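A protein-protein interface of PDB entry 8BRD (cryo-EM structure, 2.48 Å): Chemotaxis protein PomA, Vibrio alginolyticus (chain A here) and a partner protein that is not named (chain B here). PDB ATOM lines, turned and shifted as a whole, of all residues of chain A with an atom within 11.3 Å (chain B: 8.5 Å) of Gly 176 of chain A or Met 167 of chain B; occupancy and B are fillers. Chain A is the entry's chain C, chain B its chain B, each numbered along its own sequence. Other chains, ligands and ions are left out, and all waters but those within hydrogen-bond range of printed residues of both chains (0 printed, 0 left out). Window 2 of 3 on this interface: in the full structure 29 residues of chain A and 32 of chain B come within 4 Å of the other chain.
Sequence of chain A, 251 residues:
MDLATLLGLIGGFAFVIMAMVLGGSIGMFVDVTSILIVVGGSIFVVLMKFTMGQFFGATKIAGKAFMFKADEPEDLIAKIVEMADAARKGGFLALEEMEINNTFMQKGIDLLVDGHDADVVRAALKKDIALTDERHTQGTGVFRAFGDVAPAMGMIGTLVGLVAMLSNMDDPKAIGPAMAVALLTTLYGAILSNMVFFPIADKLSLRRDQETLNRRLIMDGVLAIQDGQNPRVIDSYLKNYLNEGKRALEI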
ATOM      1  N   LEU A  22      19.874 -27.404  22.324  1.00  0.00           N
ATOM      2  CA  LEU A  22      21.230 -27.767  21.925  1.00  0.00           C
ATOM      3  C   LEU A  22      21.633 -27.047  20.645  1.00  0.00           C
ATOM      4  O   LEU A  22      22.742 -26.512  20.539  1.00  0.00           O
ATOM      5  CB  LEU A  22      21.359 -29.280  21.739  1.00  0.00           C
ATOM      6  CG  LEU A  22      22.026 -30.088  22.855  1.00  0.00           C
ATOM      7  CD1 LEU A  22      22.558 -31.389  22.298  1.00  0.00           C
ATOM      8  CD2 LEU A  22      23.131 -29.312  23.537  1.00  0.00           C
ATOM      9  N   GLY A  23      20.741 -27.018  19.661  1.00  0.00           N
ATOM     10  CA  GLY A  23      21.088 -26.434  18.386  1.00  0.00           C
ATOM     11  C   GLY A  23      20.694 -24.987  18.183  1.00  0.00           C
ATOM     12  O   GLY A  23      20.804 -24.465  17.071  1.00  0.00           O
ATOM     13  N   GLY A  24      20.231 -24.327  19.240  1.00  0.00           N
ATOM     14  CA  GLY A  24      19.826 -22.940  19.129  1.00  0.00           C
ATOM     15  C   GLY A  24      18.467 -22.761  18.486  1.00  0.00           C
ATOM     16  O   GLY A  24      17.601 -22.072  19.033  1.00  0.00           O
ATOM     17  N   SER A  25      18.266 -23.379  17.323  1.00  0.00           N
ATOM     18  CA  SER A  25      16.996 -23.289  16.615  1.00  0.00           C
ATOM     19  C   SER A  25      16.410 -24.674  16.368  1.00  0.00           C
ATOM     20  O   SER A  25      16.955 -25.680  16.832  1.00  0.00           O
ATOM     21  CB  SER A  25      17.176 -22.540  15.295  1.00  0.00           C
ATOM     22  OG  SER A  25      17.541 -23.423  14.252  1.00  0.00           O
ATOM     23  N   MET A  28      16.801 -26.165  11.723  1.00  0.00           N
ATOM     24  CA  MET A  28      17.908 -26.917  11.154  1.00  0.00           C
ATOM     25  C   MET A  28      17.742 -28.423  11.315  1.00  0.00           C
ATOM     26  O   MET A  28      18.472 -29.182  10.668  1.00  0.00           O
ATOM     27  CB  MET A  28      19.222 -26.482  11.797  1.00  0.00           C
ATOM     28  CG  MET A  28      19.614 -27.338  12.961  1.00  0.00           C
ATOM     29  SD  MET A  28      20.639 -26.505  14.158  1.00  0.00           S
ATOM     30  CE  MET A  28      20.682 -27.796  15.371  1.00  0.00           C
ATOM     31  N   ASP A  31      14.378 -30.508   7.249  1.00  0.00           N
ATOM     32  CA  ASP A  31      14.884 -30.411   5.888  1.00  0.00           C
ATOM     33  C   ASP A  31      13.882 -31.096   4.978  1.00  0.00           C
ATOM     34  O   ASP A  31      13.588 -32.279   5.164  1.00  0.00           O
ATOM     35  CB  ASP A  31      16.268 -31.052   5.760  1.00  0.00           C
ATOM     36  CG  ASP A  31      16.859 -30.898   4.378  1.00  0.00           C
ATOM     37  OD1 ASP A  31      17.286 -29.776   4.038  1.00  0.00           O
ATOM     38  OD2 ASP A  31      16.905 -31.896   3.631  1.00  0.00           O
ATOM     39  N   THR A 158      21.221 -40.227   3.524  1.00  0.00           N
ATOM     40  CA  THR A 158      22.503 -39.732   4.014  1.00  0.00           C
ATOM     41  C   THR A 158      23.598 -39.928   2.974  1.00  0.00           C
ATOM     42  O   THR A 158      24.473 -39.075   2.827  1.00  0.00           O
ATOM     43  CB  THR A 158      22.859 -40.417   5.338  1.00  0.00           C
ATOM     44  OG1 THR A 158      22.042 -39.871   6.379  1.00  0.00           O
ATOM     45  CG2 THR A 158      24.318 -40.192   5.705  1.00  0.00           C
ATOM     46  N   GLY A 161      23.090 -37.123   0.611  1.00  0.00           N
ATOM     47  CA  GLY A 161      23.595 -35.885   1.176  1.00  0.00           C
ATOM     48  C   GLY A 161      25.109 -35.820   1.204  1.00  0.00           C
ATOM     49  O   GLY A 161      25.695 -34.758   1.003  1.00  0.00           O
ATOM     50  N   LEU A 162      25.760 -36.948   1.469  1.00  0.00           N
ATOM     51  CA  LEU A 162      27.217 -36.991   1.456  1.00  0.00           C
ATOM     52  C   LEU A 162      27.762 -36.764   0.057  1.00  0.00           C
ATOM     53  O   LEU A 162      28.760 -36.060  -0.115  1.00  0.00           O
ATOM     54  CB  LEU A 162      27.706 -38.325   2.012  1.00  0.00           C
ATOM     55  CG  LEU A 162      27.511 -38.526   3.512  1.00  0.00           C
ATOM     56  CD1 LEU A 162      27.644 -39.992   3.873  1.00  0.00           C
ATOM     57  CD2 LEU A 162      28.498 -37.687   4.282  1.00  0.00           C
ATOM     58  N   ALA A 164      26.252 -35.026  -2.224  1.00  0.00           N
ATOM     59  CA  ALA A 164      26.032 -33.601  -2.456  1.00  0.00           C
ATOM     60  C   ALA A 164      27.098 -32.753  -1.774  1.00  0.00           C
ATOM     61  O   ALA A 164      27.605 -31.793  -2.365  1.00  0.00           O
ATOM     62  CB  ALA A 164      24.641 -33.201  -1.975  1.00  0.00           C
ATOM     63  N   MET A 165      27.445 -33.089  -0.531  1.00  0.00           N
ATOM     64  CA  MET A 165      28.437 -32.320   0.214  1.00  0.00           C
ATOM     65  C   MET A 165      29.821 -32.452  -0.404  1.00  0.00           C
ATOM     66  O   MET A 165      30.572 -31.473  -0.487  1.00  0.00           O
ATOM     67  CB  MET A 165      28.457 -32.770   1.675  1.00  0.00           C
ATOM     68  CG  MET A 165      29.514 -32.092   2.520  1.00  0.00           C
ATOM     69  SD  MET A 165      30.076 -33.075   3.919  1.00  0.00           S
ATOM     70  CE  MET A 165      30.214 -34.695   3.181  1.00  0.00           C
ATOM     71  N   LEU A 166      30.182 -33.659  -0.842  1.00  0.00           N
ATOM     72  CA  LEU A 166      31.511 -33.875  -1.397  1.00  0.00           C
ATOM     73  C   LEU A 166      31.647 -33.251  -2.779  1.00  0.00           C
ATOM     74  O   LEU A 166      32.720 -32.756  -3.133  1.00  0.00           O
ATOM     75  CB  LEU A 166      31.823 -35.368  -1.441  1.00  0.00           C
ATOM     76  CG  LEU A 166      31.944 -36.067  -0.085  1.00  0.00           C
ATOM     77  CD1 LEU A 166      31.950 -37.568  -0.263  1.00  0.00           C
ATOM     78  CD2 LEU A 166      33.184 -35.611   0.654  1.00  0.00           C
ATOM     79  N   ASN A 168      30.444 -30.505  -3.741  1.00  0.00           N
ATOM     80  CA  ASN A 168      30.634 -29.075  -3.538  1.00  0.00           C
ATOM     81  C   ASN A 168      31.692 -28.793  -2.478  1.00  0.00           C
ATOM     82  O   ASN A 168      31.609 -27.797  -1.758  1.00  0.00           O
ATOM     83  CB  ASN A 168      29.312 -28.411  -3.159  1.00  0.00           C
ATOM     84  CG  ASN A 168      28.223 -28.665  -4.178  1.00  0.00           C
ATOM     85  OD1 ASN A 168      27.214 -29.304  -3.879  1.00  0.00           O
ATOM     86  ND2 ASN A 168      28.423 -28.172  -5.393  1.00  0.00           N
ATOM     87  N   MET A 169      32.690 -29.664  -2.372  1.00  0.00           N
ATOM     88  CA  MET A 169      33.710 -29.568  -1.334  1.00  0.00           C
ATOM     89  C   MET A 169      34.989 -29.006  -1.944  1.00  0.00           C
ATOM     90  O   MET A 169      35.744 -29.724  -2.605  1.00  0.00           O
ATOM     91  CB  MET A 169      33.964 -30.925  -0.690  1.00  0.00           C
ATOM     92  CG  MET A 169      34.825 -30.841   0.552  1.00  0.00           C
ATOM     93  SD  MET A 169      34.943 -32.396   1.442  1.00  0.00           S
ATOM     94  CE  MET A 169      36.359 -33.112   0.626  1.00  0.00           C
ATOM     95  N   ASP A 170      35.227 -27.719  -1.717  1.00  0.00           N
ATOM     96  CA  ASP A 170      36.509 -27.081  -1.985  1.00  0.00           C
ATOM     97  C   ASP A 170      37.011 -26.502  -0.673  1.00  0.00           C
ATOM     98  O   ASP A 170      36.309 -25.704  -0.041  1.00  0.00           O
ATOM     99  CB  ASP A 170      36.377 -25.984  -3.043  1.00  0.00           C
ATOM    100  CG  ASP A 170      36.223 -26.539  -4.442  1.00  0.00           C
ATOM    101  OD1 ASP A 170      36.240 -27.780  -4.595  1.00  0.00           O
ATOM    102  OD2 ASP A 170      36.082 -25.739  -5.391  1.00  0.00           O
ATOM    103  N   ASP A 171      38.217 -26.909  -0.259  1.00  0.00           N
ATOM    104  CA  ASP A 171      38.785 -26.455   1.007  1.00  0.00           C
ATOM    105  C   ASP A 171      37.835 -26.812   2.142  1.00  0.00           C
ATOM    106  O   ASP A 171      37.140 -25.935   2.669  1.00  0.00           O
ATOM    107  CB  ASP A 171      39.072 -24.953   0.979  1.00  0.00           C
ATOM    108  CG  ASP A 171      40.065 -24.570  -0.101  1.00  0.00           C
ATOM    109  OD1 ASP A 171      39.658 -24.467  -1.277  1.00  0.00           O
ATOM    110  OD2 ASP A 171      41.256 -24.380   0.225  1.00  0.00           O
ATOM    111  N   PRO A 172      37.768 -28.088   2.539  1.00  0.00           N
ATOM    112  CA  PRO A 172      36.647 -28.555   3.365  1.00  0.00           C
ATOM    113  C   PRO A 172      36.855 -27.817   4.677  1.00  0.00           C
ATOM    114  O   PRO A 172      37.644 -28.244   5.526  1.00  0.00           O
ATOM    115  CB  PRO A 172      36.868 -30.070   3.412  1.00  0.00           C
ATOM    116  CG  PRO A 172      38.342 -30.228   3.272  1.00  0.00           C
ATOM    117  CD  PRO A 172      38.791 -29.129   2.349  1.00  0.00           C
ATOM    118  N   LYS A 173      36.136 -26.710   4.857  1.00  0.00           N
ATOM    119  CA  LYS A 173      36.083 -26.046   6.152  1.00  0.00           C
ATOM    120  C   LYS A 173      34.707 -25.394   6.169  1.00  0.00           C
ATOM    121  O   LYS A 173      34.430 -24.589   7.066  1.00  0.00           O
ATOM    122  CB  LYS A 173      37.166 -25.022   6.505  1.00  0.00           C
ATOM    123  CG  LYS A 173      37.263 -23.852   5.551  1.00  0.00           C
ATOM    124  CD  LYS A 173      38.434 -22.950   5.911  1.00  0.00           C
ATOM    125  CE  LYS A 173      38.510 -22.704   7.409  1.00  0.00           C
ATOM    126  NZ  LYS A 173      39.897 -22.400   7.855  1.00  0.00           N
ATOM    127  N   ALA A 174      33.844 -25.715   5.204  1.00  0.00           N
ATOM    128  CA  ALA A 174      32.460 -25.265   5.193  1.00  0.00           C
ATOM    129  C   ALA A 174      31.486 -26.425   5.028  1.00  0.00           C
ATOM    130  O   ALA A 174      30.297 -26.191   4.787  1.00  0.00           O
ATOM    131  CB  ALA A 174      32.232 -24.233   4.084  1.00  0.00           C
ATOM    132  N   ILE A 175      31.959 -27.669   5.155  1.00  0.00           N
ATOM    133  CA  ILE A 175      31.113 -28.841   4.936  1.00  0.00           C
ATOM    134  C   ILE A 175      30.290 -29.224   6.151  1.00  0.00           C
ATOM    135  O   ILE A 175      29.550 -30.214   6.091  1.00  0.00           O
ATOM    136  CB  ILE A 175      31.962 -30.057   4.517  1.00  0.00           C
ATOM    137  CG1 ILE A 175      32.839 -30.518   5.681  1.00  0.00           C
ATOM    138  CG2 ILE A 175      32.810 -29.717   3.312  1.00  0.00           C
ATOM    139  CD1 ILE A 175      33.510 -31.843   5.448  1.00  0.00           C
ATOM    140  N   GLY A 176      30.399 -28.484   7.250  1.00  0.00           N
ATOM    141  CA  GLY A 176      29.669 -28.775   8.461  1.00  0.00           C
ATOM    142  C   GLY A 176      28.165 -28.830   8.279  1.00  0.00           C
ATOM    143  O   GLY A 176      27.527 -29.851   8.549  1.00  0.00           O
ATOM    144  N   PRO A 177      27.561 -27.718   7.847  1.00  0.00           N
ATOM    145  CA  PRO A 177      26.103 -27.724   7.636  1.00  0.00           C
ATOM    146  C   PRO A 177      25.630 -28.752   6.626  1.00  0.00           C
ATOM    147  O   PRO A 177      24.574 -29.363   6.825  1.00  0.00           O
ATOM    148  CB  PRO A 177      25.823 -26.291   7.166  1.00  0.00           C
ATOM    149  CG  PRO A 177      26.920 -25.490   7.756  1.00  0.00           C
ATOM    150  CD  PRO A 177      28.127 -26.366   7.700  1.00  0.00           C
ATOM    151  N   ALA A 178      26.376 -28.959   5.539  1.00  0.00           N
ATOM    152  CA  ALA A 178      25.977 -29.960   4.556  1.00  0.00           C
ATOM    153  C   ALA A 178      26.036 -31.362   5.145  1.00  0.00           C
ATOM    154  O   ALA A 178      25.165 -32.198   4.875  1.00  0.00           O
ATOM    155  CB  ALA A 178      26.859 -29.855   3.315  1.00  0.00           C
ATOM    156  N   MET A 179      27.052 -31.636   5.961  1.00  0.00           N
ATOM    157  CA  MET A 179      27.140 -32.929   6.628  1.00  0.00           C
ATOM    158  C   MET A 179      26.005 -33.107   7.634  1.00  0.00           C
ATOM    159  O   MET A 179      25.462 -34.208   7.783  1.00  0.00           O
ATOM    160  CB  MET A 179      28.507 -33.067   7.301  1.00  0.00           C
ATOM    161  CG  MET A 179      28.617 -34.229   8.261  1.00  0.00           C
ATOM    162  SD  MET A 179      29.322 -35.684   7.478  1.00  0.00           S
ATOM    163  CE  MET A 179      28.000 -36.860   7.743  1.00  0.00           C
ATOM    164  N   ALA A 180      25.622 -32.027   8.320  1.00  0.00           N
ATOM    165  CA  ALA A 180      24.479 -32.088   9.228  1.00  0.00           C
ATOM    166  C   ALA A 180      23.188 -32.393   8.478  1.00  0.00           C
ATOM    167  O   ALA A 180      22.367 -33.197   8.937  1.00  0.00           O
ATOM    168  CB  ALA A 180      24.352 -30.774   9.996  1.00  0.00           C
ATOM    169  N   VAL A 181      22.992 -31.759   7.322  1.00  0.00           N
ATOM    170  CA  VAL A 181      21.815 -32.046   6.507  1.00  0.00           C
ATOM    171  C   VAL A 181      21.831 -33.495   6.038  1.00  0.00           C
ATOM    172  O   VAL A 181      20.791 -34.164   6.004  1.00  0.00           O
ATOM    173  CB  VAL A 181      21.727 -31.063   5.322  1.00  0.00           C
ATOM    174  CG1 VAL A 181      20.583 -31.439   4.409  1.00  0.00           C
ATOM    175  CG2 VAL A 181      21.553 -29.643   5.826  1.00  0.00           C
ATOM    176  N   ALA A 182      23.009 -34.003   5.670  1.00  0.00           N
ATOM    177  CA  ALA A 182      23.120 -35.409   5.291  1.00  0.00           C
ATOM    178  C   ALA A 182      22.741 -36.328   6.447  1.00  0.00           C
ATOM    179  O   ALA A 182      22.062 -37.341   6.247  1.00  0.00           O
ATOM    180  CB  ALA A 182      24.538 -35.708   4.809  1.00  0.00           C
ATOM    181  N   LEU A 183      23.173 -35.988   7.664  1.00  0.00           N
ATOM    182  CA  LEU A 183      22.847 -36.779   8.847  1.00  0.00           C
ATOM    183  C   LEU A 183      21.377 -36.696   9.235  1.00  0.00           C
ATOM    184  O   LEU A 183      20.878 -37.599   9.916  1.00  0.00           O
ATOM    185  CB  LEU A 183      23.702 -36.330  10.027  1.00  0.00           C
ATOM    186  CG  LEU A 183      25.155 -36.783  10.043  1.00  0.00           C
ATOM    187  CD1 LEU A 183      25.847 -36.239  11.277  1.00  0.00           C
ATOM    188  CD2 LEU A 183      25.228 -38.297   9.997  1.00  0.00           C
ATOM    189  N   LEU A 184      20.693 -35.615   8.851  1.00  0.00           N
ATOM    190  CA  LEU A 184      19.281 -35.463   9.188  1.00  0.00           C
ATOM    191  C   LEU A 184      18.437 -36.629   8.690  1.00  0.00           C
ATOM    192  O   LEU A 184      17.454 -37.000   9.332  1.00  0.00           O
ATOM    193  CB  LEU A 184      18.735 -34.163   8.603  1.00  0.00           C
ATOM    194  CG  LEU A 184      18.724 -32.931   9.501  1.00  0.00           C
ATOM    195  CD1 LEU A 184      18.019 -31.806   8.783  1.00  0.00           C
ATOM    196  CD2 LEU A 184      18.057 -33.239  10.824  1.00  0.00           C
ATOM    197  N   LEU B 160      25.236 -34.428  16.821  1.00  0.00           N
ATOM    198  CA  LEU B 160      26.112 -34.133  15.695  1.00  0.00           C
ATOM    199  C   LEU B 160      25.473 -33.131  14.747  1.00  0.00           C
ATOM    200  O   LEU B 160      26.161 -32.256  14.219  1.00  0.00           O
ATOM    201  CB  LEU B 160      26.485 -35.420  14.963  1.00  0.00           C
ATOM    202  CG  LEU B 160      27.418 -36.356  15.739  1.00  0.00           C
ATOM    203  CD1 LEU B 160      27.849 -37.534  14.887  1.00  0.00           C
ATOM    204  CD2 LEU B 160      28.617 -35.606  16.292  1.00  0.00           C
ATOM    205  N   VAL B 161      24.159 -33.226  14.525  1.00  0.00           N
ATOM    206  CA  VAL B 161      23.492 -32.179  13.760  1.00  0.00           C
ATOM    207  C   VAL B 161      23.643 -30.837  14.463  1.00  0.00           C
ATOM    208  O   VAL B 161      23.977 -29.827  13.827  1.00  0.00           O
ATOM    209  CB  VAL B 161      22.013 -32.531  13.523  1.00  0.00           C
ATOM    210  CG1 VAL B 161      21.305 -31.379  12.832  1.00  0.00           C
ATOM    211  CG2 VAL B 161      21.892 -33.790  12.689  1.00  0.00           C
ATOM    212  N   ALA B 162      23.443 -30.809  15.787  1.00  0.00           N
ATOM    213  CA  ALA B 162      23.598 -29.564  16.528  1.00  0.00           C
ATOM    214  C   ALA B 162      25.023 -29.029  16.461  1.00  0.00           C
ATOM    215  O   ALA B 162      25.218 -27.818  16.326  1.00  0.00           O
ATOM    216  CB  ALA B 162      23.171 -29.761  17.980  1.00  0.00           C
ATOM    217  N   MET B 163      26.026 -29.900  16.549  1.00  0.00           N
ATOM    218  CA  MET B 163      27.412 -29.451  16.527  1.00  0.00           C
ATOM    219  C   MET B 163      27.815 -28.938  15.151  1.00  0.00           C
ATOM    220  O   MET B 163      28.413 -27.865  15.032  1.00  0.00           O
ATOM    221  CB  MET B 163      28.341 -30.586  16.962  1.00  0.00           C
ATOM    222  CG  MET B 163      29.750 -30.136  17.304  1.00  0.00           C
ATOM    223  SD  MET B 163      30.975 -31.447  17.133  1.00  0.00           S
ATOM    224  CE  MET B 163      30.393 -32.282  15.660  1.00  0.00           C
ATOM    225  N   LEU B 164      27.490 -29.691  14.100  1.00  0.00           N
ATOM    226  CA  LEU B 164      27.887 -29.298  12.755  1.00  0.00           C
ATOM    227  C   LEU B 164      27.119 -28.075  12.275  1.00  0.00           C
ATOM    228  O   LEU B 164      27.602 -27.348  11.403  1.00  0.00           O
ATOM    229  CB  LEU B 164      27.688 -30.465  11.793  1.00  0.00           C
ATOM    230  CG  LEU B 164      28.376 -31.778  12.171  1.00  0.00           C
ATOM    231  CD1 LEU B 164      27.743 -32.935  11.431  1.00  0.00           C
ATOM    232  CD2 LEU B 164      29.863 -31.724  11.904  1.00  0.00           C
ATOM    233  N   SER B 165      25.929 -27.831  12.828  1.00  0.00           N
ATOM    234  CA  SER B 165      25.161 -26.663  12.417  1.00  0.00           C
ATOM    235  C   SER B 165      25.686 -25.368  13.028  1.00  0.00           C
ATOM    236  O   SER B 165      25.657 -24.326  12.366  1.00  0.00           O
ATOM    237  CB  SER B 165      23.696 -26.859  12.781  1.00  0.00           C
ATOM    238  OG  SER B 165      23.157 -27.981  12.110  1.00  0.00           O
ATOM    239  N   ASN B 166      26.169 -25.406  14.268  1.00  0.00           N
ATOM    240  CA  ASN B 166      26.655 -24.221  14.969  1.00  0.00           C
ATOM    241  C   ASN B 166      28.171 -24.239  15.130  1.00  0.00           C
ATOM    242  O   ASN B 166      28.701 -23.940  16.200  1.00  0.00           O
ATOM    243  CB  ASN B 166      25.981 -24.058  16.331  1.00  0.00           C
ATOM    244  CG  ASN B 166      24.572 -24.604  16.358  1.00  0.00           C
ATOM    245  OD1 ASN B 166      24.258 -25.507  17.127  1.00  0.00           O
ATOM    246  ND2 ASN B 166      23.711 -24.051  15.515  1.00  0.00           N
ATOM    247  N   MET B 167      28.880 -24.610  14.063  1.00  0.00           N
ATOM    248  CA  MET B 167      30.338 -24.665  14.115  1.00  0.00           C
ATOM    249  C   MET B 167      30.947 -23.317  14.474  1.00  0.00           C
ATOM    250  O   MET B 167      32.011 -23.265  15.100  1.00  0.00           O
ATOM    251  CB  MET B 167      30.889 -25.137  12.774  1.00  0.00           C
ATOM    252  CG  MET B 167      31.979 -26.166  12.896  1.00  0.00           C
ATOM    253  SD  MET B 167      31.354 -27.793  13.320  1.00  0.00           S
ATOM    254  CE  MET B 167      31.425 -28.555  11.707  1.00  0.00           C
ATOM    255  N   ASP B 168      30.301 -22.221  14.085  1.00  0.00           N
ATOM    256  CA  ASP B 168      30.794 -20.887  14.398  1.00  0.00           C
ATOM    257  C   ASP B 168      30.457 -20.451  15.818  1.00  0.00           C
ATOM    258  O   ASP B 168      30.844 -19.349  16.217  1.00  0.00           O
ATOM    259  CB  ASP B 168      30.235 -19.871  13.400  1.00  0.00           C
ATOM    260  CG  ASP B 168      30.551 -20.233  11.961  1.00  0.00           C
ATOM    261  OD1 ASP B 168      31.482 -21.034  11.739  1.00  0.00           O
ATOM    262  OD2 ASP B 168      29.872 -19.714  11.052  1.00  0.00           O
ATOM    263  N   ASP B 169      29.751 -21.282  16.580  1.00  0.00           N
ATOM    264  CA  ASP B 169      29.390 -20.982  17.965  1.00  0.00           C
ATOM    265  C   ASP B 169      30.092 -21.981  18.873  1.00  0.00           C
ATOM    266  O   ASP B 169      29.573 -23.091  19.094  1.00  0.00           O
ATOM    267  CB  ASP B 169      27.877 -21.052  18.159  1.00  0.00           C
ATOM    268  CG  ASP B 169      27.428 -20.419  19.457  1.00  0.00           C
ATOM    269  OD1 ASP B 169      28.275 -19.813  20.142  1.00  0.00           O
ATOM    270  OD2 ASP B 169      26.232 -20.535  19.798  1.00  0.00           O
ATOM    271  N   PRO B 170      31.268 -21.648  19.408  1.00  0.00           N
ATOM    272  CA  PRO B 170      31.987 -22.622  20.249  1.00  0.00           C
ATOM    273  C   PRO B 170      31.206 -23.083  21.468  1.00  0.00           C
ATOM    274  O   PRO B 170      31.250 -24.270  21.810  1.00  0.00           O
ATOM    275  CB  PRO B 170      33.264 -21.862  20.632  1.00  0.00           C
ATOM    276  CG  PRO B 170      33.458 -20.884  19.527  1.00  0.00           C
ATOM    277  CD  PRO B 170      32.079 -20.449  19.134  1.00  0.00           C
ATOM    278  N   LYS B 171      30.472 -22.184  22.130  1.00  0.00           N
ATOM    279  CA  LYS B 171      29.755 -22.571  23.340  1.00  0.00           C
ATOM    280  C   LYS B 171      28.583 -23.504  23.060  1.00  0.00           C
ATOM    281  O   LYS B 171      28.034 -24.078  24.005  1.00  0.00           O
ATOM    282  CB  LYS B 171      29.265 -21.331  24.091  1.00  0.00           C
ATOM    283  CG  LYS B 171      28.884 -20.163  23.206  1.00  0.00           C
ATOM    284  CD  LYS B 171      27.943 -19.213  23.931  1.00  0.00           C
ATOM    285  CE  LYS B 171      28.041 -17.799  23.381  1.00  0.00           C
ATOM    286  NZ  LYS B 171      28.099 -17.776  21.894  1.00  0.00           N
ATOM    287  N   ALA B 172      28.186 -23.665  21.801  1.00  0.00           N
ATOM    288  CA  ALA B 172      27.192 -24.662  21.433  1.00  0.00           C
ATOM    289  C   ALA B 172      27.810 -25.969  20.960  1.00  0.00           C
ATOM    290  O   ALA B 172      27.127 -26.996  20.964  1.00  0.00           O
ATOM    291  CB  ALA B 172      26.269 -24.117  20.336  1.00  0.00           C
ATOM    292  N   ILE B 173      29.082 -25.945  20.555  1.00  0.00           N
ATOM    293  CA  ILE B 173      29.760 -27.151  20.089  1.00  0.00           C
ATOM    294  C   ILE B 173      29.949 -28.144  21.227  1.00  0.00           C
ATOM    295  O   ILE B 173      29.700 -29.343  21.067  1.00  0.00           O
ATOM    296  CB  ILE B 173      31.103 -26.772  19.440  1.00  0.00           C
ATOM    297  CG1 ILE B 173      30.870 -26.109  18.084  1.00  0.00           C
ATOM    298  CG2 ILE B 173      31.993 -27.992  19.292  1.00  0.00           C
ATOM    299  CD1 ILE B 173      32.127 -25.575  17.452  1.00  0.00           C
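OG of Ser 165 of chain B lies close to SD of Met 28 of chain A, 3.6 Å away. The side-chain amide nitrogen (ND2) of Asn 166 of chain B is in hydrogen-bond range of the backbone carbonyl oxygen (O) of Gly 23 of chain A, 3.3 Å away.
The backbone carbonyl oxygen (O) of Val 161 of chain B lies within hydrogen-bond range of the side-chain hydroxyl (OG) of Ser 165 of chain B. The side-chain amide oxygen of Asn 166 of chain B lies close to the backbone carbonyl oxygen of Ala 162 of chain B (2.6 Å).
Leu 22 of chain A touches Asn 166 of chain B. Ala 162 of chain B touches Gly 23 of chain A. CA of Ala 162 of chain B touches CE of Met 28 of chain A, at 3.6 Å. O of Gly 176 of chain A touches CB of Leu 164 of chain B, 3.3 Å away. CE of Met 167 of chain B touches CA of Gly 176 of chain A, 3.7 Å away. Pro 177 of chain A touches Leu 164 of chain B. Leu 164 of chain B touches Met 179 of chain A. Leu 164 of chain B touches Ala 180 of chain A (CB to CB, 3.8 Å). Ala 180 of chain A touches Ser 165 of chain B (CB to OG, 3.7 Å). Leu 183 of chain A touches Leu 164 of chain B (CD1 to CD1, 3.8 Å).
Of the printed residues of chain B, Gly 176 of chain A touches Leu 164 (3.3 Å) and Met 167 (3.7 Å). Of the printed residues of chain B, Ala 180 of chain A touches Val 161, Leu 164 and Ser 165. Of the printed residues of chain B, Leu 183 of chain A touches Leu 160 and Leu 164. Leu 184 of chain A touches none of the printed residues of chain B. Of the printed residues of chain A, Leu 160 of chain B touches Leu 183. Of the printed residues of chain A, Val 161 of chain B touches Ala 180. No residue of chain A comes within 4 Å of Met 163 of chain B. Printed residues of chain A within 4 Å of Ser 165 of chain B: Met 28 and Ala 180. Printed residues of chain A within 4 Å of Met 167 of chain B: Gly 176 (3.7 Å). No residue of chain A comes within 4 Å of Asp 168 of chain B. Lys 171 of chain B touches none of the printed residues of chain A. The nearest residue of chain A that does not touch Met 167 of chain B is Pro 177 of chain A (5.5 Å).
Of the 14 printed residues of chain B, 7 touch a printed residue of chain A. Along chain A the printed residues that touch a printed residue of chain B span positions 22 to 183. Among the printed residues, no Asp or Glu carboxylate lies within 4 Å of a Lys or Arg side-chain nitrogen of the other chain.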
